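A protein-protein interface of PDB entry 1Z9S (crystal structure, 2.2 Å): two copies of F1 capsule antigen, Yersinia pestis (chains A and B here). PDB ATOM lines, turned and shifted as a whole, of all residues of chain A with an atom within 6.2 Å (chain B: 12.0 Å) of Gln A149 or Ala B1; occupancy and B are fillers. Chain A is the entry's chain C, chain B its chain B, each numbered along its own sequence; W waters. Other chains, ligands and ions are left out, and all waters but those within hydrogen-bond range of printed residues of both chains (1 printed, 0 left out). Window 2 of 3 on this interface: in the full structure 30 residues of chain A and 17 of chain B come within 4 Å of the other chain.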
ATOM      1  N   ILE A  19     -11.892 -29.207  13.227  1.00  0.00           N
ATOM      2  CA  ILE A  19     -11.762 -27.864  12.586  1.00  0.00           C
ATOM      3  C   ILE A  19     -10.307 -27.532  12.243  1.00  0.00           C
ATOM      4  O   ILE A  19      -9.410 -27.642  13.083  1.00  0.00           O
ATOM      5  CB  ILE A  19     -12.309 -26.741  13.503  1.00  0.00           C
ATOM      6  CG1 ILE A  19     -13.822 -26.903  13.702  1.00  0.00           C
ATOM      7  CG2 ILE A  19     -12.002 -25.378  12.887  1.00  0.00           C
ATOM      8  CD1 ILE A  19     -14.656 -26.774  12.423  1.00  0.00           C
ATOM      9  N   GLY A  50     -13.569 -28.490   7.941  1.00  0.00           N
ATOM     10  CA  GLY A  50     -14.011 -29.444   8.946  1.00  0.00           C
ATOM     11  C   GLY A  50     -15.324 -29.180   9.654  1.00  0.00           C
ATOM     12  O   GLY A  50     -15.678 -29.900  10.589  1.00  0.00           O
ATOM     13  N   TYR A  51     -16.054 -28.157   9.236  1.00  0.00           N
ATOM     14  CA  TYR A  51     -17.322 -27.864   9.881  1.00  0.00           C
ATOM     15  C   TYR A  51     -18.438 -28.778   9.379  1.00  0.00           C
ATOM     16  O   TYR A  51     -18.389 -29.294   8.262  1.00  0.00           O
ATOM     17  CB  TYR A  51     -17.690 -26.395   9.677  1.00  0.00           C
ATOM     18  CG  TYR A  51     -17.465 -25.897   8.270  1.00  0.00           C
ATOM     19  CD1 TYR A  51     -18.410 -26.128   7.266  1.00  0.00           C
ATOM     20  CD2 TYR A  51     -16.300 -25.196   7.941  1.00  0.00           C
ATOM     21  CE1 TYR A  51     -18.197 -25.667   5.960  1.00  0.00           C
ATOM     22  CE2 TYR A  51     -16.075 -24.736   6.648  1.00  0.00           C
ATOM     23  CZ  TYR A  51     -17.026 -24.972   5.662  1.00  0.00           C
ATOM     24  OH  TYR A  51     -16.801 -24.513   4.386  1.00  0.00           O
ATOM     25  N   LYS A  52     -19.440 -28.973  10.228  1.00  0.00           N
ATOM     26  CA  LYS A  52     -20.575 -29.830   9.920  1.00  0.00           C
ATOM     27  C   LYS A  52     -21.354 -29.331   8.707  1.00  0.00           C
ATOM     28  O   LYS A  52     -21.222 -28.179   8.300  1.00  0.00           O
ATOM     29  CB  LYS A  52     -21.505 -29.913  11.141  1.00  0.00           C
ATOM     30  CG  LYS A  52     -22.574 -30.996  11.042  1.00  0.00           C
ATOM     31  CD  LYS A  52     -23.386 -31.133  12.329  1.00  0.00           C
ATOM     32  CE  LYS A  52     -24.245 -29.905  12.587  1.00  0.00           C
ATOM     33  NZ  LYS A  52     -25.134 -30.091  13.767  1.00  0.00           N
ATOM     34  N   THR A  55     -23.211 -25.617   8.282  1.00  0.00           N
ATOM     35  CA  THR A  55     -22.667 -24.577   9.151  1.00  0.00           C
ATOM     36  C   THR A  55     -22.777 -23.260   8.380  1.00  0.00           C
ATOM     37  O   THR A  55     -22.440 -23.194   7.195  1.00  0.00           O
ATOM     38  CB  THR A  55     -21.177 -24.846   9.502  1.00  0.00           C
ATOM     39  OG1 THR A  55     -21.088 -25.977  10.383  1.00  0.00           O
ATOM     40  CG2 THR A  55     -20.554 -23.628  10.184  1.00  0.00           C
ATOM     41  N   SER A  59     -22.047 -18.650  12.671  1.00  0.00           N
ATOM     42  CA  SER A  59     -21.512 -19.610  13.639  1.00  0.00           C
ATOM     43  C   SER A  59     -19.978 -19.595  13.655  1.00  0.00           C
ATOM     44  O   SER A  59     -19.344 -20.296  14.451  1.00  0.00           O
ATOM     45  CB  SER A  59     -22.013 -21.021  13.330  1.00  0.00           C
ATOM     46  OG  SER A  59     -23.401 -21.110  13.586  1.00  0.00           O
ATOM     47  N   VAL A 146     -15.882 -22.144  16.023  1.00  0.00           N
ATOM     48  CA  VAL A 146     -17.061 -22.509  15.245  1.00  0.00           C
ATOM     49  C   VAL A 146     -18.104 -23.096  16.184  1.00  0.00           C
ATOM     50  O   VAL A 146     -17.841 -24.086  16.871  1.00  0.00           O
ATOM     51  CB  VAL A 146     -16.734 -23.555  14.158  1.00  0.00           C
ATOM     52  CG1 VAL A 146     -17.939 -23.734  13.239  1.00  0.00           C
ATOM     53  CG2 VAL A 146     -15.517 -23.119  13.354  1.00  0.00           C
ATOM     54  N   SER A 147     -19.284 -22.484  16.208  1.00  0.00           N
ATOM     55  CA  SER A 147     -20.364 -22.933  17.077  1.00  0.00           C
ATOM     56  C   SER A 147     -21.355 -23.868  16.388  1.00  0.00           C
ATOM     57  O   SER A 147     -21.299 -24.079  15.168  1.00  0.00           O
ATOM     58  CB  SER A 147     -21.116 -21.724  17.635  1.00  0.00           C
ATOM     59  OG  SER A 147     -20.274 -20.934  18.456  1.00  0.00           O
ATOM     60  N   ASN A 148     -22.262 -24.426  17.185  1.00  0.00           N
ATOM     61  CA  ASN A 148     -23.284 -25.334  16.679  1.00  0.00           C
ATOM     62  C   ASN A 148     -22.688 -26.497  15.899  1.00  0.00           C
ATOM     63  O   ASN A 148     -23.206 -26.879  14.849  1.00  0.00           O
ATOM     64  CB  ASN A 148     -24.262 -24.569  15.787  1.00  0.00           C
ATOM     65  CG  ASN A 148     -24.832 -23.346  16.474  1.00  0.00           C
ATOM     66  OD1 ASN A 148     -25.391 -23.438  17.566  1.00  0.00           O
ATOM     67  ND2 ASN A 148     -24.695 -22.193  15.838  1.00  0.00           N
ATOM     68  N   GLN A 149     -21.597 -27.058  16.405  1.00  0.00           N
ATOM     69  CA  GLN A 149     -20.972 -28.181  15.724  1.00  0.00           C
ATOM     70  C   GLN A 149     -21.463 -29.496  16.315  1.00  0.00           C
ATOM     71  O   GLN A 149     -20.615 -30.359  16.614  1.00  0.00           O
ATOM     72  CB  GLN A 149     -19.448 -28.079  15.832  1.00  0.00           C
ATOM     73  CG  GLN A 149     -18.890 -26.874  15.099  1.00  0.00           C
ATOM     74  CD  GLN A 149     -19.315 -26.861  13.650  1.00  0.00           C
ATOM     75  OE1 GLN A 149     -18.925 -27.735  12.868  1.00  0.00           O
ATOM     76  NE2 GLN A 149     -20.131 -25.879  13.282  1.00  0.00           N
ATOM     77  OXT GLN A 149     -22.695 -29.649  16.460  1.00  0.00           O
ATOM     78  N   ALA B   1     -22.113 -27.312  19.619  1.00  0.00           N
ATOM     79  CA  ALA B   1     -20.814 -27.329  20.351  1.00  0.00           C
ATOM     80  C   ALA B   1     -19.801 -26.431  19.655  1.00  0.00           C
ATOM     81  O   ALA B   1     -19.890 -26.199  18.447  1.00  0.00           O
ATOM     82  CB  ALA B   1     -20.280 -28.750  20.423  1.00  0.00           C
ATOM     83  N   ASP B   2     -18.832 -25.940  20.423  1.00  0.00           N
ATOM     84  CA  ASP B   2     -17.791 -25.053  19.901  1.00  0.00           C
ATOM     85  C   ASP B   2     -16.468 -25.766  19.620  1.00  0.00           C
ATOM     86  O   ASP B   2     -15.887 -26.407  20.497  1.00  0.00           O
ATOM     87  CB  ASP B   2     -17.533 -23.909  20.889  1.00  0.00           C
ATOM     88  CG  ASP B   2     -18.741 -23.007  21.072  1.00  0.00           C
ATOM     89  OD1 ASP B   2     -18.668 -22.089  21.916  1.00  0.00           O
ATOM     90  OD2 ASP B   2     -19.760 -23.206  20.376  1.00  0.00           O
ATOM     91  N   LEU B   3     -15.998 -25.644  18.385  1.00  0.00           N
ATOM     92  CA  LEU B   3     -14.730 -26.240  17.978  1.00  0.00           C
ATOM     93  C   LEU B   3     -13.809 -25.082  17.604  1.00  0.00           C
ATOM     94  O   LEU B   3     -14.262 -24.073  17.063  1.00  0.00           O
ATOM     95  CB  LEU B   3     -14.929 -27.186  16.783  1.00  0.00           C
ATOM     96  CG  LEU B   3     -15.676 -28.497  17.065  1.00  0.00           C
ATOM     97  CD1 LEU B   3     -15.874 -29.279  15.777  1.00  0.00           C
ATOM     98  CD2 LEU B   3     -14.889 -29.326  18.071  1.00  0.00           C
ATOM     99  N   THR B   4     -12.521 -25.224  17.895  1.00  0.00           N
ATOM    100  CA  THR B   4     -11.582 -24.154  17.608  1.00  0.00           C
ATOM    101  C   THR B   4     -10.327 -24.606  16.881  1.00  0.00           C
ATOM    102  O   THR B   4      -9.987 -25.790  16.851  1.00  0.00           O
ATOM    103  CB  THR B   4     -11.121 -23.466  18.900  1.00  0.00           C
ATOM    104  OG1 THR B   4     -10.096 -24.256  19.513  1.00  0.00           O
ATOM    105  CG2 THR B   4     -12.283 -23.327  19.879  1.00  0.00           C
ATOM    106  N   ALA B   5      -9.643 -23.627  16.302  1.00  0.00           N
ATOM    107  CA  ALA B   5      -8.398 -23.836  15.583  1.00  0.00           C
ATOM    108  C   ALA B   5      -7.745 -22.461  15.554  1.00  0.00           C
ATOM    109  O   ALA B   5      -8.434 -21.443  15.654  1.00  0.00           O
ATOM    110  CB  ALA B   5      -8.675 -24.334  14.165  1.00  0.00           C
HETATM  111  O   HOH W   1     -22.248 -24.371  19.934  1.00  0.00           O
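O of Leu B3 sits at hydrogen-bond distance from N of Val A146 (2.7 Å). The side-chain carboxylate (OD2) of Asp B2 lies within hydrogen-bond range of the side-chain hydroxyl (OG) of Ser A147, at 3.0 Å. The backbone NH (N) of Gln A149 sits at hydrogen-bond distance from the backbone carbonyl oxygen (O) of Ala B1, 2.8 Å away. The backbone NH of Asn A148 lies within hydrogen-bond range of the backbone carbonyl oxygen of Ala B1. O of Val A146 lies close to O of Ala B1, 3.3 Å away.
The backbone carbonyl oxygen (O) of Ser A59 lies within hydrogen-bond range of the backbone NH (N) of Ser A147, at 2.8 Å. The side-chain amide nitrogen (ND2) of Asn A148 sits at hydrogen-bond distance from the side-chain hydroxyl (OG) of Ser A59 (2.8 Å). The side-chain hydroxyl of Thr A55 is in hydrogen-bond range of the side-chain amide nitrogen of Gln A149, 3.1 Å away. The backbone carbonyl oxygen of Ser A147 is in hydrogen-bond range of the side-chain amide nitrogen of Gln A149 (2.9 Å). OXT of Gln A149 lies within salt-bridge range of NZ of Lys A52, 3.7 Å away.
Leu B3 touches Ile A19 (CB to CG1, 3.3 Å). O of Ile A19 touches CB of Ala B5, 3.6 Å away. Val A146 touches Asp B2. O of Ala B1 touches C of Ser A147, at 3.4 Å. Gln A149 touches Leu B3.
Of chain B, only Ala B1 and Leu B3 come within 4 Å of Gln A149. Of chain A, only Val A146 (3.3 Å), Ser A147 (3.4 Å), Asn A148 (3.2 Å) and Gln A149 (2.8 Å) come within 4 Å of Ala B1. No residue of chain B comes within 4 Å of Thr A55. No residue of chain B comes within 4 Å of Ser A59. Of chain B, only Ala B1 (3.3 Å), Asp B2 (3.2 Å) and Leu B3 (2.7 Å) come within 4 Å of Val A146. Ser A147 touches just these residues of chain B: Ala B1 and Asp B2. Of chain B, only Ala B1 (3.2 Å) comes within 4 Å of Asn A148. Of the printed residues of chain B, Ile A19 touches Leu B3 and Ala B5. Printed residues of chain A within 4 Å of Leu B3: Ile A19, Val A146 and Gln A149. Printed residues of chain A within 4 Å of Ala B5: Ile A19 (3.6 Å). Printed residues of chain A within 4 Å of Asp B2: Val A146 (3.2 Å) and Ser A147 (3.0 Å). Thr B4 touches none of the printed residues of chain A. Tyr A51 touches none of the printed residues of chain B. The nearest printed residue of chain A that does not touch Ala B1 is Lys A52 (7.1 Å).
Printed residues of chain A that touch a printed residue of chain B: Ile A19, Val A146, Ser A147, Asn A148 and Gln A149. Hydrophobic or aromatic side chains of chain A that line the printed part of chain B: Ile A19 and Val A146. Of the 5 printed residues of chain B, 4 touch a printed residue of chain A. Among the printed residues, 10 pairs touch across the chains. Among the printed residues, no Asp or Glu carboxylate lies within 4 Å of a Lys or Arg side-chain nitrogen of the other chain.
No position is printed for both chains. Of the 10 pairs that touch across the chains among the printed residues, none has its exchanged pair printed and touching as well.
Water W1 lies within hydrogen-bond range of the backbone NH of Asn A148 (2.7 Å), the side-chain carboxylate of Asp B2 (2.8 Å) and the backbone NH of Ala B1 (3.0 Å).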
